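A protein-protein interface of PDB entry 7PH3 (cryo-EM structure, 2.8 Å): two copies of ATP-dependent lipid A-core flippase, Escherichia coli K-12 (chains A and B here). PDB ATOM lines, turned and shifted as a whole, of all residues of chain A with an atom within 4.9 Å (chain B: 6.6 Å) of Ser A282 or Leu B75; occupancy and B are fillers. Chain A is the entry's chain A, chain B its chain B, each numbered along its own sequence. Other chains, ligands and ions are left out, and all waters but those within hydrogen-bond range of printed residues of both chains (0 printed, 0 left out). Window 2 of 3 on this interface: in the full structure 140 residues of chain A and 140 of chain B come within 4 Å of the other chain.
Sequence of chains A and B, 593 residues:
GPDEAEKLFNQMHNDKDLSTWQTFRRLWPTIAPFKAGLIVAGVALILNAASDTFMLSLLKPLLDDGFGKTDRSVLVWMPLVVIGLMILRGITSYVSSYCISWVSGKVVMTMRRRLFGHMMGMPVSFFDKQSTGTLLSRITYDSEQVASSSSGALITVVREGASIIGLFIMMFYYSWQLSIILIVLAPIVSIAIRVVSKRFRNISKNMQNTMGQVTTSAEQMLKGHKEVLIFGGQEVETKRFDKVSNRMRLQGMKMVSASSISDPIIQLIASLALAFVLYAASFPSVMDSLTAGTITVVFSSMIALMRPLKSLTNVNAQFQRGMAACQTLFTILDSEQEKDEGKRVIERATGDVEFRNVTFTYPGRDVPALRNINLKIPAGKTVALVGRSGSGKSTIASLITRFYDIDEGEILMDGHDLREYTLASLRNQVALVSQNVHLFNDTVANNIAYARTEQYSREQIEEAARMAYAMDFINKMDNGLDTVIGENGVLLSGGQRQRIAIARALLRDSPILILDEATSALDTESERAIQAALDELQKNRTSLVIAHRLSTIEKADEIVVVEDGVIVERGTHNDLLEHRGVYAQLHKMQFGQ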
ATOM      1  N   LEU A 278     -24.604 -14.318  -6.413  1.00  0.00           N
ATOM      2  CA  LEU A 278     -23.436 -14.101  -7.259  1.00  0.00           C
ATOM      3  C   LEU A 278     -23.765 -14.312  -8.733  1.00  0.00           C
ATOM      4  O   LEU A 278     -23.304 -13.553  -9.594  1.00  0.00           O
ATOM      5  CB  LEU A 278     -22.288 -15.003  -6.818  1.00  0.00           C
ATOM      6  CG  LEU A 278     -21.728 -14.722  -5.422  1.00  0.00           C
ATOM      7  CD1 LEU A 278     -20.692 -15.760  -5.015  1.00  0.00           C
ATOM      8  CD2 LEU A 278     -21.139 -13.328  -5.360  1.00  0.00           C
ATOM      9  N   TYR A 279     -24.564 -15.330  -9.050  1.00  0.00           N
ATOM     10  CA  TYR A 279     -24.935 -15.539 -10.445  1.00  0.00           C
ATOM     11  C   TYR A 279     -25.801 -14.397 -10.965  1.00  0.00           C
ATOM     12  O   TYR A 279     -25.646 -13.964 -12.112  1.00  0.00           O
ATOM     13  CB  TYR A 279     -25.650 -16.876 -10.614  1.00  0.00           C
ATOM     14  CG  TYR A 279     -25.573 -17.421 -12.021  1.00  0.00           C
ATOM     15  CD1 TYR A 279     -24.520 -18.227 -12.414  1.00  0.00           C
ATOM     16  CD2 TYR A 279     -26.550 -17.123 -12.955  1.00  0.00           C
ATOM     17  CE1 TYR A 279     -24.445 -18.730 -13.700  1.00  0.00           C
ATOM     18  CE2 TYR A 279     -26.484 -17.616 -14.242  1.00  0.00           C
ATOM     19  CZ  TYR A 279     -25.430 -18.419 -14.611  1.00  0.00           C
ATOM     20  OH  TYR A 279     -25.356 -18.917 -15.892  1.00  0.00           O
ATOM     21  N   ALA A 280     -26.720 -13.903 -10.140  1.00  0.00           N
ATOM     22  CA  ALA A 280     -27.546 -12.776 -10.547  1.00  0.00           C
ATOM     23  C   ALA A 280     -26.697 -11.542 -10.794  1.00  0.00           C
ATOM     24  O   ALA A 280     -26.933 -10.798 -11.752  1.00  0.00           O
ATOM     25  CB  ALA A 280     -28.608 -12.492  -9.486  1.00  0.00           C
ATOM     26  N   ALA A 281     -25.701 -11.309  -9.939  1.00  0.00           N
ATOM     27  CA  ALA A 281     -24.796 -10.192 -10.164  1.00  0.00           C
ATOM     28  C   ALA A 281     -24.031 -10.361 -11.467  1.00  0.00           C
ATOM     29  O   ALA A 281     -23.874  -9.402 -12.232  1.00  0.00           O
ATOM     30  CB  ALA A 281     -23.832 -10.052  -8.988  1.00  0.00           C
ATOM     31  N   SER A 282     -23.548 -11.573 -11.741  1.00  0.00           N
ATOM     32  CA  SER A 282     -22.822 -11.809 -12.985  1.00  0.00           C
ATOM     33  C   SER A 282     -23.715 -11.634 -14.208  1.00  0.00           C
ATOM     34  O   SER A 282     -23.230 -11.240 -15.274  1.00  0.00           O
ATOM     35  CB  SER A 282     -22.213 -13.209 -12.985  1.00  0.00           C
ATOM     36  OG  SER A 282     -23.058 -14.122 -13.664  1.00  0.00           O
ATOM     37  N   PHE A 283     -25.003 -11.930 -14.077  1.00  0.00           N
ATOM     38  CA  PHE A 283     -25.910 -11.833 -15.213  1.00  0.00           C
ATOM     39  C   PHE A 283     -25.982 -10.388 -15.700  1.00  0.00           C
ATOM     40  O   PHE A 283     -26.104  -9.466 -14.886  1.00  0.00           O
ATOM     41  CB  PHE A 283     -27.301 -12.330 -14.824  1.00  0.00           C
ATOM     42  CG  PHE A 283     -28.071 -12.934 -15.959  1.00  0.00           C
ATOM     43  CD1 PHE A 283     -27.620 -14.084 -16.583  1.00  0.00           C
ATOM     44  CD2 PHE A 283     -29.252 -12.360 -16.393  1.00  0.00           C
ATOM     45  CE1 PHE A 283     -28.330 -14.644 -17.626  1.00  0.00           C
ATOM     46  CE2 PHE A 283     -29.967 -12.915 -17.434  1.00  0.00           C
ATOM     47  CZ  PHE A 283     -29.506 -14.059 -18.052  1.00  0.00           C
ATOM     48  N   PRO A 284     -25.939 -10.154 -17.013  1.00  0.00           N
ATOM     49  CA  PRO A 284     -25.741  -8.795 -17.534  1.00  0.00           C
ATOM     50  C   PRO A 284     -26.986  -7.924 -17.562  1.00  0.00           C
ATOM     51  O   PRO A 284     -26.966  -6.881 -18.222  1.00  0.00           O
ATOM     52  CB  PRO A 284     -25.241  -9.060 -18.962  1.00  0.00           C
ATOM     53  CG  PRO A 284     -25.909 -10.331 -19.347  1.00  0.00           C
ATOM     54  CD  PRO A 284     -25.996 -11.158 -18.089  1.00  0.00           C
ATOM     55  N   MET A 287     -27.543  -5.762 -12.707  1.00  0.00           N
ATOM     56  CA  MET A 287     -26.867  -4.637 -12.080  1.00  0.00           C
ATOM     57  C   MET A 287     -27.289  -3.334 -12.756  1.00  0.00           C
ATOM     58  O   MET A 287     -28.136  -3.309 -13.654  1.00  0.00           O
ATOM     59  CB  MET A 287     -25.347  -4.803 -12.127  1.00  0.00           C
ATOM     60  CG  MET A 287     -24.682  -4.403 -13.441  1.00  0.00           C
ATOM     61  SD  MET A 287     -25.428  -5.082 -14.927  1.00  0.00           S
ATOM     62  CE  MET A 287     -24.753  -6.729 -14.850  1.00  0.00           C
ATOM     63  N   LEU B  62     -15.323  -8.837  -4.770  1.00  0.00           N
ATOM     64  CA  LEU B  62     -16.656  -8.548  -5.290  1.00  0.00           C
ATOM     65  C   LEU B  62     -16.920  -7.054  -5.360  1.00  0.00           C
ATOM     66  O   LEU B  62     -17.657  -6.594  -6.238  1.00  0.00           O
ATOM     67  CB  LEU B  62     -17.713  -9.233  -4.425  1.00  0.00           C
ATOM     68  CG  LEU B  62     -19.184  -8.907  -4.691  1.00  0.00           C
ATOM     69  CD1 LEU B  62     -19.575  -9.296  -6.103  1.00  0.00           C
ATOM     70  CD2 LEU B  62     -20.084  -9.594  -3.681  1.00  0.00           C
ATOM     71  N   ASP B  65     -13.210  -5.345  -7.665  1.00  0.00           N
ATOM     72  CA  ASP B  65     -13.489  -5.814  -9.013  1.00  0.00           C
ATOM     73  C   ASP B  65     -14.996  -5.764  -9.203  1.00  0.00           C
ATOM     74  O   ASP B  65     -15.700  -6.738  -8.923  1.00  0.00           O
ATOM     75  CB  ASP B  65     -12.947  -7.228  -9.225  1.00  0.00           C
ATOM     76  CG  ASP B  65     -12.556  -7.494 -10.661  1.00  0.00           C
ATOM     77  OD1 ASP B  65     -13.451  -7.801 -11.476  1.00  0.00           O
ATOM     78  OD2 ASP B  65     -11.351  -7.405 -10.975  1.00  0.00           O
ATOM     79  N   GLY B  66     -15.494  -4.623  -9.665  1.00  0.00           N
ATOM     80  CA  GLY B  66     -16.910  -4.341  -9.610  1.00  0.00           C
ATOM     81  C   GLY B  66     -17.741  -5.229 -10.515  1.00  0.00           C
ATOM     82  O   GLY B  66     -17.244  -6.001 -11.335  1.00  0.00           O
ATOM     83  N   PHE B  67     -19.057  -5.108 -10.336  1.00  0.00           N
ATOM     84  CA  PHE B  67     -20.000  -5.861 -11.154  1.00  0.00           C
ATOM     85  C   PHE B  67     -19.867  -5.494 -12.627  1.00  0.00           C
ATOM     86  O   PHE B  67     -19.905  -6.369 -13.499  1.00  0.00           O
ATOM     87  CB  PHE B  67     -21.425  -5.616 -10.659  1.00  0.00           C
ATOM     88  CG  PHE B  67     -21.665  -4.214 -10.168  1.00  0.00           C
ATOM     89  CD1 PHE B  67     -22.084  -3.221 -11.038  1.00  0.00           C
ATOM     90  CD2 PHE B  67     -21.467  -3.888  -8.834  1.00  0.00           C
ATOM     91  CE1 PHE B  67     -22.303  -1.932 -10.589  1.00  0.00           C
ATOM     92  CE2 PHE B  67     -21.685  -2.600  -8.380  1.00  0.00           C
ATOM     93  CZ  PHE B  67     -22.103  -1.622  -9.259  1.00  0.00           C
ATOM     94  N   GLY B  68     -19.712  -4.207 -12.923  1.00  0.00           N
ATOM     95  CA  GLY B  68     -19.512  -3.766 -14.288  1.00  0.00           C
ATOM     96  C   GLY B  68     -18.327  -2.837 -14.432  1.00  0.00           C
ATOM     97  O   GLY B  68     -17.872  -2.565 -15.548  1.00  0.00           O
ATOM     98  N   THR B  70     -15.213  -3.383 -13.474  1.00  0.00           N
ATOM     99  CA  THR B  70     -14.079  -4.172 -13.926  1.00  0.00           C
ATOM    100  C   THR B  70     -14.592  -5.343 -14.757  1.00  0.00           C
ATOM    101  O   THR B  70     -15.769  -5.706 -14.692  1.00  0.00           O
ATOM    102  CB  THR B  70     -13.246  -4.675 -12.736  1.00  0.00           C
ATOM    103  OG1 THR B  70     -13.110  -3.623 -11.773  1.00  0.00           O
ATOM    104  CG2 THR B  70     -11.851  -5.091 -13.187  1.00  0.00           C
ATOM    105  N   ASP B  71     -13.706  -6.009 -15.506  1.00  0.00           N
ATOM    106  CA  ASP B  71     -14.129  -7.234 -16.242  1.00  0.00           C
ATOM    107  C   ASP B  71     -14.849  -8.172 -15.263  1.00  0.00           C
ATOM    108  O   ASP B  71     -14.312  -8.384 -14.160  1.00  0.00           O
ATOM    109  CB  ASP B  71     -12.937  -7.925 -16.909  1.00  0.00           C
ATOM    110  CG  ASP B  71     -12.268  -7.075 -17.975  1.00  0.00           C
ATOM    111  OD1 ASP B  71     -12.805  -5.994 -18.286  1.00  0.00           O
ATOM    112  OD2 ASP B  71     -11.213  -7.503 -18.486  1.00  0.00           O
ATOM    113  N   ARG B  72     -15.992  -8.746 -15.660  1.00  0.00           N
ATOM    114  CA  ARG B  72     -16.797  -9.586 -14.727  1.00  0.00           C
ATOM    115  C   ARG B  72     -15.969 -10.786 -14.262  1.00  0.00           C
ATOM    116  O   ARG B  72     -16.070 -11.099 -13.068  1.00  0.00           O
ATOM    117  CB  ARG B  72     -18.070 -10.073 -15.425  1.00  0.00           C
ATOM    118  CG  ARG B  72     -19.049  -8.964 -15.784  1.00  0.00           C
ATOM    119  CD  ARG B  72     -19.937  -9.357 -16.948  1.00  0.00           C
ATOM    120  NE  ARG B  72     -20.459 -10.710 -16.821  1.00  0.00           N
ATOM    121  CZ  ARG B  72     -21.231 -11.307 -17.723  1.00  0.00           C
ATOM    122  NH1 ARG B  72     -21.656 -12.541 -17.517  1.00  0.00           N
ATOM    123  NH2 ARG B  72     -21.580 -10.665 -18.824  1.00  0.00           N
ATOM    124  N   SER B  73     -15.166 -11.392 -15.151  1.00  0.00           N
ATOM    125  CA  SER B  73     -14.236 -12.518 -14.832  1.00  0.00           C
ATOM    126  C   SER B  73     -14.497 -13.256 -13.510  1.00  0.00           C
ATOM    127  O   SER B  73     -14.962 -14.408 -13.575  1.00  0.00           O
ATOM    128  CB  SER B  73     -12.804 -12.045 -14.903  1.00  0.00           C
ATOM    129  OG  SER B  73     -12.527 -11.471 -16.172  1.00  0.00           O
ATOM    130  N   VAL B  74     -14.174 -12.651 -12.362  1.00  0.00           N
ATOM    131  CA  VAL B  74     -14.283 -13.374 -11.055  1.00  0.00           C
ATOM    132  C   VAL B  74     -15.732 -13.810 -10.817  1.00  0.00           C
ATOM    133  O   VAL B  74     -15.930 -14.950 -10.350  1.00  0.00           O
ATOM    134  CB  VAL B  74     -13.775 -12.485  -9.902  1.00  0.00           C
ATOM    135  CG1 VAL B  74     -13.773 -13.221  -8.570  1.00  0.00           C
ATOM    136  CG2 VAL B  74     -12.399 -11.910 -10.198  1.00  0.00           C
ATOM    137  N   LEU B  75     -16.701 -12.948 -11.134  1.00  0.00           N
ATOM    138  CA  LEU B  75     -18.135 -13.258 -10.890  1.00  0.00           C
ATOM    139  C   LEU B  75     -18.513 -14.616 -11.490  1.00  0.00           C
ATOM    140  O   LEU B  75     -19.459 -15.235 -10.963  1.00  0.00           O
ATOM    141  CB  LEU B  75     -18.987 -12.142 -11.501  1.00  0.00           C
ATOM    142  CG  LEU B  75     -19.108 -10.875 -10.659  1.00  0.00           C
ATOM    143  CD1 LEU B  75     -19.768  -9.759 -11.454  1.00  0.00           C
ATOM    144  CD2 LEU B  75     -19.887 -11.153  -9.384  1.00  0.00           C
ATOM    145  N   VAL B  76     -17.819 -15.064 -12.544  1.00  0.00           N
ATOM    146  CA  VAL B  76     -18.225 -16.300 -13.199  1.00  0.00           C
ATOM    147  C   VAL B  76     -17.876 -17.505 -12.335  1.00  0.00           C
ATOM    148  O   VAL B  76     -18.702 -18.401 -12.133  1.00  0.00           O
ATOM    149  CB  VAL B  76     -17.591 -16.391 -14.600  1.00  0.00           C
ATOM    150  CG1 VAL B  76     -18.300 -17.454 -15.440  1.00  0.00           C
ATOM    151  CG2 VAL B  76     -17.603 -15.022 -15.283  1.00  0.00           C
ATOM    152  N   TRP B  77     -16.654 -17.550 -11.810  1.00  0.00           N
ATOM    153  CA  TRP B  77     -16.248 -18.680 -10.979  1.00  0.00           C
ATOM    154  C   TRP B  77     -16.604 -18.502  -9.509  1.00  0.00           C
ATOM    155  O   TRP B  77     -16.484 -19.458  -8.743  1.00  0.00           O
ATOM    156  CB  TRP B  77     -14.747 -18.924 -11.119  1.00  0.00           C
ATOM    157  CG  TRP B  77     -14.317 -19.400 -12.481  1.00  0.00           C
ATOM    158  CD1 TRP B  77     -13.543 -18.721 -13.371  1.00  0.00           C
ATOM    159  CD2 TRP B  77     -14.614 -20.663 -13.093  1.00  0.00           C
ATOM    160  NE1 TRP B  77     -13.347 -19.473 -14.501  1.00  0.00           N
ATOM    161  CE2 TRP B  77     -13.994 -20.671 -14.357  1.00  0.00           C
ATOM    162  CE3 TRP B  77     -15.349 -21.787 -12.699  1.00  0.00           C
ATOM    163  CZ2 TRP B  77     -14.083 -21.755 -15.230  1.00  0.00           C
ATOM    164  CZ3 TRP B  77     -15.435 -22.863 -13.570  1.00  0.00           C
ATOM    165  CH2 TRP B  77     -14.807 -22.838 -14.819  1.00  0.00           C
ATOM    166  N   MET B  78     -17.044 -17.313  -9.103  1.00  0.00           N
ATOM    167  CA  MET B  78     -17.366 -17.090  -7.696  1.00  0.00           C
ATOM    168  C   MET B  78     -18.452 -18.006  -7.132  1.00  0.00           C
ATOM    169  O   MET B  78     -18.280 -18.471  -5.991  1.00  0.00           O
ATOM    170  CB  MET B  78     -17.739 -15.619  -7.480  1.00  0.00           C
ATOM    171  CG  MET B  78     -17.269 -15.098  -6.134  1.00  0.00           C
ATOM    172  SD  MET B  78     -17.823 -13.429  -5.744  1.00  0.00           S
ATOM    173  CE  MET B  78     -16.415 -12.763  -4.847  1.00  0.00           C
ATOM    174  N   PRO B  79     -19.580 -18.278  -7.813  1.00  0.00           N
ATOM    175  CA  PRO B  79     -20.554 -19.209  -7.213  1.00  0.00           C
ATOM    176  C   PRO B  79     -19.988 -20.598  -6.941  1.00  0.00           C
ATOM    177  O   PRO B  79     -20.286 -21.190  -5.894  1.00  0.00           O
ATOM    178  CB  PRO B  79     -21.688 -19.244  -8.249  1.00  0.00           C
ATOM    179  CG  PRO B  79     -21.556 -17.991  -9.013  1.00  0.00           C
ATOM    180  CD  PRO B  79     -20.086 -17.721  -9.079  1.00  0.00           C
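Hydrophobic or aromatic side chains of chain A within 4 Å of the printed part of chain B: Leu A278, Pro A284 and Met A287.
Of the 15 printed residues of chain B, 5 touch a printed residue of chain A.
Printed residues of chain B that touch a printed residue of chain A: Phe B67, Arg B72, Leu B75, Met B78 and Pro B79.
The side-chain hydroxyl (OG) of Ser A282 sits at hydrogen-bond distance from the backbone carbonyl oxygen (O) of Tyr A279 (3.0 Å).
No position is printed for both chains.
Of the 6 pairs that touch across the chains among the printed residues, none has its exchanged pair printed and touching as well.
Leu A278 touches Met B78 (CD2 to SD, 3.3 Å).
Leu A278 touches Pro B79 (CB to CG, 3.8 Å).
CB of Ser A282 touches CB of Leu B75, 3.7 Å away.
CB of Pro A284 touches NH2 of Arg B72 (3.9997 Å).
Phe B67 touches Met A287 (CD1 to CG, 3.7 Å).
The guanidinium group (NH1) of Arg B72 lies within hydrogen-bond range of the backbone carbonyl oxygen (O) of Ser A282 (3.0 Å).
Of the printed residues of chain B, Ser A282 touches Arg B72 (3.0 Å) and Leu B75 (3.7 Å).
Of the printed residues of chain A, Leu B75 touches Ser A282 (3.7 Å).
Of the printed residues of chain B, Leu A278 touches Met B78 and Pro B79.
Printed residues of chain A within 4 Å of Met B78: Leu A278 (3.3 Å).
Printed residues of chain B within 4 Å of Met A287: Phe B67.
Of the printed residues of chain A, Arg B72 touches Ser A282 and Pro A284.
Of the printed residues of chain A, Pro B79 touches Leu A278.
Asp B71 touches none of the printed residues of chain A.
The nearest residue of chain A that does not touch Leu B75 is Ala A281 (4.1 Å).
The nearest printed residue of chain B that does not touch Pro A284 is Phe B67 (7.5 Å).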
